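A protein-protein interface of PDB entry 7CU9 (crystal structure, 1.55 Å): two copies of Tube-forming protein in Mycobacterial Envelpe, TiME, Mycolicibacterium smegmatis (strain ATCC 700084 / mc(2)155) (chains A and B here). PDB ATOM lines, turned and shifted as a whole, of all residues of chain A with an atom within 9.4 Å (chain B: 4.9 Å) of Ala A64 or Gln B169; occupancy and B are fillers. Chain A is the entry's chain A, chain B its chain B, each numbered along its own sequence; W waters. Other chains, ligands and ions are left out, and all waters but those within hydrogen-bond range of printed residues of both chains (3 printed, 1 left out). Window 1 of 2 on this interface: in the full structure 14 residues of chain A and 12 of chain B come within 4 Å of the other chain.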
ATOM      1  N   SER A   3      -4.331 -15.362  31.525  1.00  0.00           N
ATOM      2  CA  SER A   3      -3.172 -15.796  30.709  1.00  0.00           C
ATOM      3  C   SER A   3      -2.740 -14.664  29.777  1.00  0.00           C
ATOM      4  O   SER A   3      -3.612 -13.964  29.222  1.00  0.00           O
ATOM      5  CB  SER A   3      -3.494 -17.028  29.913  1.00  0.00           C
ATOM      6  OG  SER A   3      -3.746 -18.138  30.762  1.00  0.00           O
ATOM      7  N   ASP A   4      -1.433 -14.542  29.570  1.00  0.00           N
ATOM      8  CA  ASP A   4      -0.859 -13.686  28.503  1.00  0.00           C
ATOM      9  C   ASP A   4      -1.063 -14.401  27.171  1.00  0.00           C
ATOM     10  O   ASP A   4      -1.169 -15.627  27.129  1.00  0.00           O
ATOM     11  CB  ASP A   4       0.615 -13.396  28.769  1.00  0.00           C
ATOM     12  CG  ASP A   4       0.864 -12.532  29.992  1.00  0.00           C
ATOM     13  OD1 ASP A   4       0.008 -11.693  30.311  1.00  0.00           O
ATOM     14  OD2 ASP A   4       1.920 -12.720  30.616  1.00  0.00           O
ATOM     15  N   PRO A   5      -1.123 -13.669  26.036  1.00  0.00           N
ATOM     16  CA  PRO A   5      -1.334 -14.300  24.733  1.00  0.00           C
ATOM     17  C   PRO A   5      -0.272 -15.350  24.372  1.00  0.00           C
ATOM     18  O   PRO A   5      -0.574 -16.285  23.626  1.00  0.00           O
ATOM     19  CB  PRO A   5      -1.295 -13.156  23.707  1.00  0.00           C
ATOM     20  CG  PRO A   5      -1.106 -11.871  24.492  1.00  0.00           C
ATOM     21  CD  PRO A   5      -1.075 -12.202  25.967  1.00  0.00           C
ATOM     22  N   GLY A   6       0.942 -15.199  24.904  1.00  0.00           N
ATOM     23  CA  GLY A   6       2.073 -16.092  24.602  1.00  0.00           C
ATOM     24  C   GLY A   6       1.819 -17.536  25.010  1.00  0.00           C
ATOM     25  O   GLY A   6       2.547 -18.412  24.511  1.00  0.00           O
ATOM     26  N   VAL A   7       0.858 -17.807  25.894  1.00  0.00           N
ATOM     27  CA  VAL A   7       0.698 -19.188  26.449  1.00  0.00           C
ATOM     28  C   VAL A   7       0.347 -20.164  25.322  1.00  0.00           C
ATOM     29  O   VAL A   7       0.605 -21.361  25.502  1.00  0.00           O
ATOM     30  CB  VAL A   7      -0.319 -19.278  27.604  1.00  0.00           C
ATOM     31  CG1 VAL A   7       0.097 -18.413  28.782  1.00  0.00           C
ATOM     32  CG2 VAL A   7      -1.743 -18.978  27.164  1.00  0.00           C
ATOM     33  N   VAL A   8      -0.219 -19.701  24.202  1.00  0.00           N
ATOM     34  CA  VAL A   8      -0.654 -20.622  23.107  1.00  0.00           C
ATOM     35  C   VAL A   8       0.562 -21.370  22.543  1.00  0.00           C
ATOM     36  O   VAL A   8       0.369 -22.499  22.049  1.00  0.00           O
ATOM     37  CB  VAL A   8      -1.447 -19.910  21.993  1.00  0.00           C
ATOM     38  CG1 VAL A   8      -2.745 -19.315  22.510  1.00  0.00           C
ATOM     39  CG2 VAL A   8      -0.627 -18.860  21.274  1.00  0.00           C
ATOM     40  N   THR A  33      -2.233 -21.748  13.258  1.00  0.00           N
ATOM     41  CA  THR A  33      -2.109 -20.482  14.022  1.00  0.00           C
ATOM     42  C   THR A  33      -3.377 -19.638  13.865  1.00  0.00           C
ATOM     43  O   THR A  33      -3.387 -18.503  14.352  1.00  0.00           O
ATOM     44  CB  THR A  33      -0.858 -19.716  13.576  1.00  0.00           C
ATOM     45  OG1 THR A  33      -0.971 -19.493  12.172  1.00  0.00           O
ATOM     46  CG2 THR A  33       0.415 -20.474  13.881  1.00  0.00           C
ATOM     47  N   PRO A  35      -7.991 -20.094  13.624  1.00  0.00           N
ATOM     48  CA  PRO A  35      -9.164 -20.959  13.584  1.00  0.00           C
ATOM     49  C   PRO A  35      -9.468 -21.294  12.120  1.00  0.00           C
ATOM     50  O   PRO A  35      -9.231 -20.475  11.239  1.00  0.00           O
ATOM     51  CB  PRO A  35     -10.279 -20.125  14.223  1.00  0.00           C
ATOM     52  CG  PRO A  35      -9.554 -19.082  15.042  1.00  0.00           C
ATOM     53  CD  PRO A  35      -8.255 -18.823  14.310  1.00  0.00           C
ATOM     54  N   PHE A  58     -14.078 -19.084  17.800  1.00  0.00           N
ATOM     55  CA  PHE A  58     -12.866 -18.368  18.278  1.00  0.00           C
ATOM     56  C   PHE A  58     -12.732 -16.969  17.675  1.00  0.00           C
ATOM     57  O   PHE A  58     -12.314 -16.073  18.421  1.00  0.00           O
ATOM     58  CB  PHE A  58     -11.609 -19.178  17.985  1.00  0.00           C
ATOM     59  CG  PHE A  58     -11.403 -20.301  18.959  1.00  0.00           C
ATOM     60  CD1 PHE A  58     -10.774 -20.071  20.171  1.00  0.00           C
ATOM     61  CD2 PHE A  58     -11.848 -21.582  18.671  1.00  0.00           C
ATOM     62  CE1 PHE A  58     -10.584 -21.104  21.074  1.00  0.00           C
ATOM     63  CE2 PHE A  58     -11.672 -22.609  19.584  1.00  0.00           C
ATOM     64  CZ  PHE A  58     -11.033 -22.372  20.778  1.00  0.00           C
ATOM     65  N   ASN A  59     -13.006 -16.781  16.387  1.00  0.00           N
ATOM     66  CA  ASN A  59     -12.753 -15.463  15.752  1.00  0.00           C
ATOM     67  C   ASN A  59     -13.651 -14.430  16.428  1.00  0.00           C
ATOM     68  O   ASN A  59     -14.851 -14.691  16.619  1.00  0.00           O
ATOM     69  CB  ASN A  59     -12.904 -15.495  14.236  1.00  0.00           C
ATOM     70  CG  ASN A  59     -11.667 -16.029  13.553  1.00  0.00           C
ATOM     71  OD1 ASN A  59     -10.546 -15.773  13.990  1.00  0.00           O
ATOM     72  ND2 ASN A  59     -11.862 -16.751  12.466  1.00  0.00           N
ATOM     73  N   ASP A  60     -13.060 -13.306  16.821  1.00  0.00           N
ATOM     74  CA  ASP A  60     -13.725 -12.327  17.707  1.00  0.00           C
ATOM     75  C   ASP A  60     -12.841 -11.095  17.804  1.00  0.00           C
ATOM     76  O   ASP A  60     -11.621 -11.217  17.764  1.00  0.00           O
ATOM     77  CB  ASP A  60     -13.927 -12.927  19.096  1.00  0.00           C
ATOM     78  CG  ASP A  60     -14.825 -12.081  19.968  1.00  0.00           C
ATOM     79  OD1 ASP A  60     -16.040 -12.043  19.681  1.00  0.00           O
ATOM     80  OD2 ASP A  60     -14.297 -11.457  20.907  1.00  0.00           O
ATOM     81  N   PRO A  61     -13.412  -9.880  17.942  1.00  0.00           N
ATOM     82  CA  PRO A  61     -12.583  -8.696  18.168  1.00  0.00           C
ATOM     83  C   PRO A  61     -11.592  -8.872  19.324  1.00  0.00           C
ATOM     84  O   PRO A  61     -10.533  -8.274  19.270  1.00  0.00           O
ATOM     85  CB  PRO A  61     -13.620  -7.611  18.481  1.00  0.00           C
ATOM     86  CG  PRO A  61     -14.824  -8.046  17.682  1.00  0.00           C
ATOM     87  CD  PRO A  61     -14.843  -9.555  17.819  1.00  0.00           C
ATOM     88  N   ASP A  62     -11.933  -9.689  20.327  1.00  0.00           N
ATOM     89  CA  ASP A  62     -11.128  -9.831  21.568  1.00  0.00           C
ATOM     90  C   ASP A  62     -10.290 -11.117  21.554  1.00  0.00           C
ATOM     91  O   ASP A  62      -9.684 -11.413  22.597  1.00  0.00           O
ATOM     92  CB  ASP A  62     -12.029  -9.722  22.796  1.00  0.00           C
ATOM     93  CG  ASP A  62     -12.469  -8.290  23.025  1.00  0.00           C
ATOM     94  OD1 ASP A  62     -11.603  -7.394  22.917  1.00  0.00           O
ATOM     95  OD2 ASP A  62     -13.663  -8.082  23.282  1.00  0.00           O
ATOM     96  N   LEU A  63     -10.197 -11.832  20.429  1.00  0.00           N
ATOM     97  CA  LEU A  63      -9.242 -12.969  20.325  1.00  0.00           C
ATOM     98  C   LEU A  63      -7.823 -12.396  20.229  1.00  0.00           C
ATOM     99  O   LEU A  63      -7.495 -11.755  19.215  1.00  0.00           O
ATOM    100  CB  LEU A  63      -9.569 -13.866  19.129  1.00  0.00           C
ATOM    101  CG  LEU A  63      -8.687 -15.111  19.013  1.00  0.00           C
ATOM    102  CD1 LEU A  63      -8.855 -16.036  20.216  1.00  0.00           C
ATOM    103  CD2 LEU A  63      -8.980 -15.853  17.725  1.00  0.00           C
ATOM    104  N   ALA A  64      -7.014 -12.601  21.267  1.00  0.00           N
ATOM    105  CA  ALA A  64      -5.636 -12.060  21.344  1.00  0.00           C
ATOM    106  C   ALA A  64      -4.669 -12.989  20.611  1.00  0.00           C
ATOM    107  O   ALA A  64      -3.773 -12.508  19.886  1.00  0.00           O
ATOM    108  CB  ALA A  64      -5.235 -11.858  22.778  1.00  0.00           C
ATOM    109  N   SER A  65      -4.794 -14.296  20.830  1.00  0.00           N
ATOM    110  CA  SER A  65      -3.870 -15.289  20.238  1.00  0.00           C
ATOM    111  C   SER A  65      -4.583 -16.624  20.101  1.00  0.00           C
ATOM    112  O   SER A  65      -5.597 -16.859  20.768  1.00  0.00           O
ATOM    113  CB  SER A  65      -2.614 -15.431  21.048  1.00  0.00           C
ATOM    114  OG  SER A  65      -2.916 -15.918  22.339  1.00  0.00           O
ATOM    115  N   PHE A  66      -4.051 -17.461  19.234  1.00  0.00           N
ATOM    116  CA  PHE A  66      -4.668 -18.760  18.918  1.00  0.00           C
ATOM    117  C   PHE A  66      -3.596 -19.687  18.375  1.00  0.00           C
ATOM    118  O   PHE A  66      -2.787 -19.259  17.536  1.00  0.00           O
ATOM    119  CB  PHE A  66      -5.797 -18.578  17.908  1.00  0.00           C
ATOM    120  CG  PHE A  66      -6.490 -19.870  17.571  1.00  0.00           C
ATOM    121  CD1 PHE A  66      -7.552 -20.324  18.341  1.00  0.00           C
ATOM    122  CD2 PHE A  66      -6.057 -20.647  16.514  1.00  0.00           C
ATOM    123  CE1 PHE A  66      -8.188 -21.518  18.039  1.00  0.00           C
ATOM    124  CE2 PHE A  66      -6.692 -21.841  16.215  1.00  0.00           C
ATOM    125  CZ  PHE A  66      -7.747 -22.280  16.985  1.00  0.00           C
ATOM    126  N   GLY A  67      -3.618 -20.931  18.837  1.00  0.00           N
ATOM    127  CA  GLY A  67      -2.762 -21.993  18.295  1.00  0.00           C
ATOM    128  C   GLY A  67      -3.441 -23.334  18.414  1.00  0.00           C
ATOM    129  O   GLY A  67      -4.271 -23.519  19.318  1.00  0.00           O
ATOM    130  N   VAL A  86      -6.342 -23.740  21.230  1.00  0.00           N
ATOM    131  CA  VAL A  86      -6.245 -22.862  22.426  1.00  0.00           C
ATOM    132  C   VAL A  86      -6.383 -21.420  21.958  1.00  0.00           C
ATOM    133  O   VAL A  86      -5.605 -21.010  21.086  1.00  0.00           O
ATOM    134  CB  VAL A  86      -4.931 -23.074  23.192  1.00  0.00           C
ATOM    135  CG1 VAL A  86      -4.861 -22.173  24.416  1.00  0.00           C
ATOM    136  CG2 VAL A  86      -4.723 -24.534  23.579  1.00  0.00           C
ATOM    137  N   GLY A  87      -7.347 -20.701  22.527  1.00  0.00           N
ATOM    138  CA  GLY A  87      -7.557 -19.269  22.262  1.00  0.00           C
ATOM    139  C   GLY A  87      -7.393 -18.468  23.532  1.00  0.00           C
ATOM    140  O   GLY A  87      -7.992 -18.838  24.562  1.00  0.00           O
ATOM    141  N   VAL A  88      -6.591 -17.406  23.473  1.00  0.00           N
ATOM    142  CA  VAL A  88      -6.461 -16.436  24.591  1.00  0.00           C
ATOM    143  C   VAL A  88      -7.234 -15.184  24.194  1.00  0.00           C
ATOM    144  O   VAL A  88      -6.958 -14.638  23.115  1.00  0.00           O
ATOM    145  CB  VAL A  88      -4.997 -16.106  24.906  1.00  0.00           C
ATOM    146  CG1 VAL A  88      -4.918 -15.085  26.034  1.00  0.00           C
ATOM    147  CG2 VAL A  88      -4.205 -17.365  25.236  1.00  0.00           C
ATOM    148  N   PHE A  89      -8.182 -14.774  25.030  1.00  0.00           N
ATOM    149  CA  PHE A  89      -9.021 -13.576  24.796  1.00  0.00           C
ATOM    150  C   PHE A  89      -8.532 -12.416  25.668  1.00  0.00           C
ATOM    151  O   PHE A  89      -7.923 -12.630  26.722  1.00  0.00           O
ATOM    152  CB  PHE A  89     -10.490 -13.912  25.036  1.00  0.00           C
ATOM    153  CG  PHE A  89     -11.026 -14.908  24.041  1.00  0.00           C
ATOM    154  CD1 PHE A  89     -10.836 -16.268  24.235  1.00  0.00           C
ATOM    155  CD2 PHE A  89     -11.667 -14.486  22.887  1.00  0.00           C
ATOM    156  CE1 PHE A  89     -11.316 -17.184  23.308  1.00  0.00           C
ATOM    157  CE2 PHE A  89     -12.137 -15.404  21.957  1.00  0.00           C
ATOM    158  CZ  PHE A  89     -11.960 -16.751  22.172  1.00  0.00           C
ATOM    159  N   ALA A  90      -8.807 -11.194  25.218  1.00  0.00           N
ATOM    160  CA  ALA A  90      -8.389  -9.952  25.909  1.00  0.00           C
ATOM    161  C   ALA A  90      -9.122  -9.823  27.246  1.00  0.00           C
ATOM    162  O   ALA A  90      -8.578  -9.179  28.160  1.00  0.00           O
ATOM    163  CB  ALA A  90      -8.640  -8.758  25.027  1.00  0.00           C
ATOM    164  N   THR A  91     -10.310 -10.412  27.367  1.00  0.00           N
ATOM    165  CA  THR A  91     -11.136 -10.333  28.596  1.00  0.00           C
ATOM    166  C   THR A  91     -11.708 -11.704  28.937  1.00  0.00           C
ATOM    167  O   THR A  91     -11.869 -12.544  28.034  1.00  0.00           O
ATOM    168  CB  THR A  91     -12.281  -9.328  28.444  1.00  0.00           C
ATOM    169  OG1 THR A  91     -13.220  -9.877  27.520  1.00  0.00           O
ATOM    170  CG2 THR A  91     -11.807  -7.969  27.978  1.00  0.00           C
ATOM    171  N   ALA A  94     -15.067 -12.189  27.100  1.00  0.00           N
ATOM    172  CA  ALA A  94     -14.933 -12.603  25.684  1.00  0.00           C
ATOM    173  C   ALA A  94     -14.721 -14.121  25.618  1.00  0.00           C
ATOM    174  O   ALA A  94     -15.314 -14.762  24.728  1.00  0.00           O
ATOM    175  CB  ALA A  94     -13.811 -11.853  25.013  1.00  0.00           C
ATOM    176  N   ALA A  95     -13.912 -14.685  26.514  1.00  0.00           N
ATOM    177  CA  ALA A  95     -13.711 -16.154  26.572  1.00  0.00           C
ATOM    178  C   ALA A  95     -15.049 -16.827  26.914  1.00  0.00           C
ATOM    179  O   ALA A  95     -15.346 -17.884  26.335  1.00  0.00           O
ATOM    180  CB  ALA A  95     -12.628 -16.516  27.555  1.00  0.00           C
ATOM    181  N   ASN A 160      -9.543 -16.198  30.884  1.00  0.00           N
ATOM    182  CA  ASN A 160      -9.645 -15.577  29.540  1.00  0.00           C
ATOM    183  C   ASN A 160      -9.237 -16.573  28.445  1.00  0.00           C
ATOM    184  O   ASN A 160      -8.973 -16.128  27.326  1.00  0.00           O
ATOM    185  CB  ASN A 160      -8.785 -14.315  29.454  1.00  0.00           C
ATOM    186  CG  ASN A 160      -7.311 -14.593  29.649  1.00  0.00           C
ATOM    187  OD1 ASN A 160      -6.932 -15.470  30.432  1.00  0.00           O
ATOM    188  ND2 ASN A 160      -6.468 -13.871  28.929  1.00  0.00           N
ATOM    189  N   VAL A 161      -9.187 -17.868  28.751  1.00  0.00           N
ATOM    190  CA  VAL A 161      -8.745 -18.906  27.777  1.00  0.00           C
ATOM    191  C   VAL A 161      -9.917 -19.832  27.457  1.00  0.00           C
ATOM    192  O   VAL A 161     -10.623 -20.257  28.380  1.00  0.00           O
ATOM    193  CB  VAL A 161      -7.539 -19.700  28.301  1.00  0.00           C
ATOM    194  CG1 VAL A 161      -7.158 -20.828  27.350  1.00  0.00           C
ATOM    195  CG2 VAL A 161      -6.353 -18.788  28.563  1.00  0.00           C
ATOM    196  N   VAL B  22       3.518 -12.548  21.333  1.00  0.00           N
ATOM    197  CA  VAL B  22       2.247 -12.536  20.542  1.00  0.00           C
ATOM    198  C   VAL B  22       1.658 -13.950  20.464  1.00  0.00           C
ATOM    199  O   VAL B  22       0.459 -14.057  20.140  1.00  0.00           O
ATOM    200  CB  VAL B  22       2.416 -11.920  19.138  1.00  0.00           C
ATOM    201  CG1 VAL B  22       2.896 -10.483  19.220  1.00  0.00           C
ATOM    202  CG2 VAL B  22       3.308 -12.740  18.224  1.00  0.00           C
ATOM    203  N   THR B  79       0.800 -11.172   8.572  1.00  0.00           N
ATOM    204  CA  THR B  79      -0.376 -11.666   9.340  1.00  0.00           C
ATOM    205  C   THR B  79      -0.270 -11.140  10.778  1.00  0.00           C
ATOM    206  O   THR B  79      -1.265 -10.576  11.293  1.00  0.00           O
ATOM    207  CB  THR B  79      -0.474 -13.195   9.285  1.00  0.00           C
ATOM    208  OG1 THR B  79      -0.730 -13.583   7.932  1.00  0.00           O
ATOM    209  CG2 THR B  79      -1.569 -13.729  10.180  1.00  0.00           C
ATOM    210  N   HIS B  80       0.890 -11.334  11.402  1.00  0.00           N
ATOM    211  CA  HIS B  80       1.322 -10.598  12.618  1.00  0.00           C
ATOM    212  C   HIS B  80       2.422  -9.632  12.184  1.00  0.00           C
ATOM    213  O   HIS B  80       3.355 -10.081  11.483  1.00  0.00           O
ATOM    214  CB  HIS B  80       1.764 -11.557  13.741  1.00  0.00           C
ATOM    215  CG  HIS B  80       0.656 -12.375  14.324  1.00  0.00           C
ATOM    216  ND1 HIS B  80      -0.051 -11.975  15.434  1.00  0.00           N
ATOM    217  CD2 HIS B  80       0.148 -13.578  13.969  1.00  0.00           C
ATOM    218  CE1 HIS B  80      -0.952 -12.891  15.736  1.00  0.00           C
ATOM    219  NE2 HIS B  80      -0.847 -13.886  14.848  1.00  0.00           N
ATOM    220  N   ASP B 148     -10.796  -6.870   9.531  1.00  0.00           N
ATOM    221  CA  ASP B 148     -10.736  -7.017  11.008  1.00  0.00           C
ATOM    222  C   ASP B 148      -9.292  -6.800  11.477  1.00  0.00           C
ATOM    223  O   ASP B 148      -8.981  -7.200  12.607  1.00  0.00           O
ATOM    224  CB  ASP B 148     -11.282  -8.376  11.450  1.00  0.00           C
ATOM    225  CG  ASP B 148     -10.490  -9.577  10.961  1.00  0.00           C
ATOM    226  OD1 ASP B 148      -9.590  -9.393  10.117  1.00  0.00           O
ATOM    227  OD2 ASP B 148     -10.784 -10.696  11.431  1.00  0.00           O
ATOM    228  N   ARG B 149      -8.432  -6.210  10.643  1.00  0.00           N
ATOM    229  CA  ARG B 149      -7.019  -5.959  11.021  1.00  0.00           C
ATOM    230  C   ARG B 149      -6.942  -4.673  11.848  1.00  0.00           C
ATOM    231  O   ARG B 149      -7.338  -3.599  11.345  1.00  0.00           O
ATOM    232  CB  ARG B 149      -6.115  -5.862   9.795  1.00  0.00           C
ATOM    233  CG  ARG B 149      -4.646  -5.697  10.154  1.00  0.00           C
ATOM    234  CD  ARG B 149      -3.798  -5.759   8.910  1.00  0.00           C
ATOM    235  NE  ARG B 149      -2.365  -5.669   9.144  1.00  0.00           N
ATOM    236  CZ  ARG B 149      -1.577  -6.664   9.547  1.00  0.00           C
ATOM    237  NH1 ARG B 149      -2.069  -7.858   9.829  1.00  0.00           N
ATOM    238  NH2 ARG B 149      -0.279  -6.443   9.680  1.00  0.00           N
ATOM    239  N   ARG B 150      -6.433  -4.779  13.074  1.00  0.00           N
ATOM    240  CA  ARG B 150      -6.255  -3.615  13.971  1.00  0.00           C
ATOM    241  C   ARG B 150      -4.814  -3.594  14.470  1.00  0.00           C
ATOM    242  O   ARG B 150      -4.248  -4.666  14.739  1.00  0.00           O
ATOM    243  CB  ARG B 150      -7.256  -3.631  15.127  1.00  0.00           C
ATOM    244  CG  ARG B 150      -8.692  -3.431  14.663  1.00  0.00           C
ATOM    245  CD  ARG B 150      -9.655  -3.189  15.796  1.00  0.00           C
ATOM    246  NE  ARG B 150      -9.759  -4.383  16.627  1.00  0.00           N
ATOM    247  CZ  ARG B 150     -10.213  -4.407  17.875  1.00  0.00           C
ATOM    248  NH1 ARG B 150     -10.640  -3.301  18.461  1.00  0.00           N
ATOM    249  NH2 ARG B 150     -10.246  -5.550  18.539  1.00  0.00           N
ATOM    250  N   VAL B 167       1.349  -3.564  17.764  1.00  0.00           N
ATOM    251  CA  VAL B 167       1.038  -4.974  17.401  1.00  0.00           C
ATOM    252  C   VAL B 167      -0.165  -4.952  16.463  1.00  0.00           C
ATOM    253  O   VAL B 167      -1.224  -4.460  16.881  1.00  0.00           O
ATOM    254  CB  VAL B 167       0.793  -5.847  18.641  1.00  0.00           C
ATOM    255  CG1 VAL B 167       0.308  -7.232  18.244  1.00  0.00           C
ATOM    256  CG2 VAL B 167       2.041  -5.942  19.509  1.00  0.00           C
ATOM    257  N   CYS B 168       0.034  -5.441  15.237  1.00  0.00           N
ATOM    258  CA  CYS B 168      -0.978  -5.474  14.156  1.00  0.00           C
ATOM    259  C   CYS B 168      -1.382  -6.928  13.918  1.00  0.00           C
ATOM    260  O   CYS B 168      -0.494  -7.792  13.818  1.00  0.00           O
ATOM    261  CB  CYS B 168      -0.437  -4.888  12.861  1.00  0.00           C
ATOM    262  SG  CYS B 168       0.047  -3.145  12.974  1.00  0.00           S
ATOM    263  N   GLN B 169      -2.683  -7.180  13.841  1.00  0.00           N
ATOM    264  CA  GLN B 169      -3.244  -8.539  13.687  1.00  0.00           C
ATOM    265  C   GLN B 169      -4.760  -8.429  13.599  1.00  0.00           C
ATOM    266  O   GLN B 169      -5.313  -7.375  13.938  1.00  0.00           O
ATOM    267  CB  GLN B 169      -2.867  -9.436  14.869  1.00  0.00           C
ATOM    268  CG  GLN B 169      -3.112  -8.800  16.233  1.00  0.00           C
ATOM    269  CD  GLN B 169      -2.926  -9.785  17.362  1.00  0.00           C
ATOM    270  OE1 GLN B 169      -1.816 -10.041  17.814  1.00  0.00           O
ATOM    271  NE2 GLN B 169      -4.028 -10.347  17.832  1.00  0.00           N
ATOM    272  N   SER B 170      -5.419  -9.505  13.183  1.00  0.00           N
ATOM    273  CA  SER B 170      -6.862  -9.668  13.446  1.00  0.00           C
ATOM    274  C   SER B 170      -7.061  -9.812  14.962  1.00  0.00           C
ATOM    275  O   SER B 170      -6.055  -9.841  15.715  1.00  0.00           O
ATOM    276  CB  SER B 170      -7.418 -10.824  12.664  1.00  0.00           C
ATOM    277  OG  SER B 170      -6.766 -12.027  13.016  1.00  0.00           O
ATOM    278  N   GLY B 171      -8.306  -9.857  15.422  1.00  0.00           N
ATOM    279  CA  GLY B 171      -8.598  -9.928  16.862  1.00  0.00           C
ATOM    280  C   GLY B 171      -8.001  -8.738  17.594  1.00  0.00           C
ATOM    281  O   GLY B 171      -8.147  -7.607  17.096  1.00  0.00           O
ATOM    282  N   ASN B 172      -7.336  -8.977  18.722  1.00  0.00           N
ATOM    283  CA  ASN B 172      -6.949  -7.905  19.678  1.00  0.00           C
ATOM    284  C   ASN B 172      -5.463  -8.019  20.018  1.00  0.00           C
ATOM    285  O   ASN B 172      -5.110  -8.862  20.860  1.00  0.00           O
ATOM    286  CB  ASN B 172      -7.810  -7.978  20.933  1.00  0.00           C
ATOM    287  CG  ASN B 172      -7.725  -6.735  21.791  1.00  0.00           C
ATOM    288  OD1 ASN B 172      -6.668  -6.118  21.900  1.00  0.00           O
ATOM    289  ND2 ASN B 172      -8.836  -6.363  22.400  1.00  0.00           N
ATOM    290  N   GLY B 173      -4.638  -7.150  19.427  1.00  0.00           N
ATOM    291  CA  GLY B 173      -3.196  -7.081  19.719  1.00  0.00           C
ATOM    292  C   GLY B 173      -2.881  -6.292  20.982  1.00  0.00           C
ATOM    293  O   GLY B 173      -1.681  -6.153  21.290  1.00  0.00           O
ATOM    294  N   PRO B 175      -3.401  -6.882  24.442  1.00  0.00           N
ATOM    295  CA  PRO B 175      -2.667  -7.595  25.485  1.00  0.00           C
ATOM    296  C   PRO B 175      -1.182  -7.776  25.133  1.00  0.00           C
ATOM    297  O   PRO B 175      -0.331  -7.546  25.982  1.00  0.00           O
ATOM    298  CB  PRO B 175      -3.424  -8.926  25.568  1.00  0.00           C
ATOM    299  CG  PRO B 175      -4.834  -8.546  25.201  1.00  0.00           C
ATOM    300  CD  PRO B 175      -4.656  -7.554  24.067  1.00  0.00           C
HETATM  301  O   HOH W   1     -11.982  -5.355  20.855  1.00  0.00           O
HETATM  302  O   HOH W   2      -1.534 -13.565  18.370  1.00  0.00           O
HETATM  303  O   HOH W   3      -2.601 -16.328  15.559  1.00  0.00           O
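NH2 of Arg B150 lies within hydrogen-bond range of O of Pro A61.
The backbone NH (N) of Asn B172 lies close to the backbone carbonyl oxygen (O) of Pro A61 (3.3 Å).
OD1 of Asp A62 lies within hydrogen-bond range of ND2 of Asn B172.
O of Leu A63 is in hydrogen-bond range of N of Asn B172 (2.8 Å).
The side-chain amide nitrogen (NE2) of Gln B169 lies within hydrogen-bond range of the backbone carbonyl oxygen (O) of Ala A64 (3.0 Å).
O of Gly B171 lies close to O of Pro A61.
The side-chain hydroxyl of Ser A65 sits at hydrogen-bond distance from the backbone carbonyl oxygen of Pro A5.
OD2 of Asp A60 is in hydrogen-bond range of N of Asp A62, at 3.0 Å.
The backbone NH of Ala A90 is in hydrogen-bond range of the backbone carbonyl oxygen of Asp A62 (2.8 Å).
N of Ala A64 lies within hydrogen-bond range of O of Val A88 (2.8 Å).
The backbone carbonyl oxygen of Ser A65 sits at hydrogen-bond distance from the backbone NH of Val A88 (2.9 Å).
The backbone carbonyl oxygen (O) of Gly B171 is in hydrogen-bond range of the guanidinium group (NH2) of Arg B150 (3.3 Å).
Pro A5 touches Pro B175 (CG to CB, 3.9 Å).
Gly B171 touches Asp A60 (CA to O, 3.4 Å).
Leu A63 touches Gln B169 (O to NE2, 3.99 Å).
Gly B171 touches Leu A63.
Ala A64 touches Asn B172 (CA to O, 3.3 Å).
Ser A65 touches Val B22.
Asn B172 touches Ala A90 (ND2 to CB, 3.6 Å).
CB of Ala A90 touches CG of Pro B175, 3.8 Å away.
Printed residues of chain B within 4 Å of Asp A62: Asn B172 (3.0 Å).
Of the printed residues of chain B, Leu A63 touches Gln B169, Gly B171 and Asn B172.
Val A161 touches none of the printed residues of chain B.
Arg B149 touches none of the printed residues of chain A.
Of the printed residues of chain A, Arg B150 touches Pro A61.
Printed residues of chain A within 4 Å of Gln B169: Leu A63 (3.99 Å) and Ala A64 (3.0 Å).
Gly B171 touches just these residues of chain A: Asp A60, Pro A61 and Leu A63.
No residue of chain A comes within 4 Å of Gly B173.
The nearest printed residue of chain A that does not touch Gln B169 is Ser A65 (5.0 Å).
The nearest printed residue of chain B that does not touch Asp A60 is Asn B172 (4.9 Å).
Printed residues of chain B that touch a printed residue of chain A: Val B22, Arg B150, Gln B169, Gly B171, Asn B172 and Pro B175.
Among the printed residues, no Asp or Glu carboxylate lies within 4 Å of a Lys or Arg side-chain nitrogen of the other chain.
No position is printed for both chains.
Of the 14 pairs that touch across the chains among the printed residues, none has its exchanged pair printed and touching as well.
Water W3 bridges the backbone carbonyl oxygen of Thr A33 (2.6 Å) and a ring nitrogen (NE2) of His B80 (3.1 Å).
Water W2 bridges the backbone carbonyl oxygen of Val B22 (2.7 Å) and the backbone carbonyl oxygen of Ala A64 (2.9 Å).
Water W1 lies within hydrogen-bond range of the guanidinium group of Arg B150 and the side-chain carboxylate of Asp A62.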
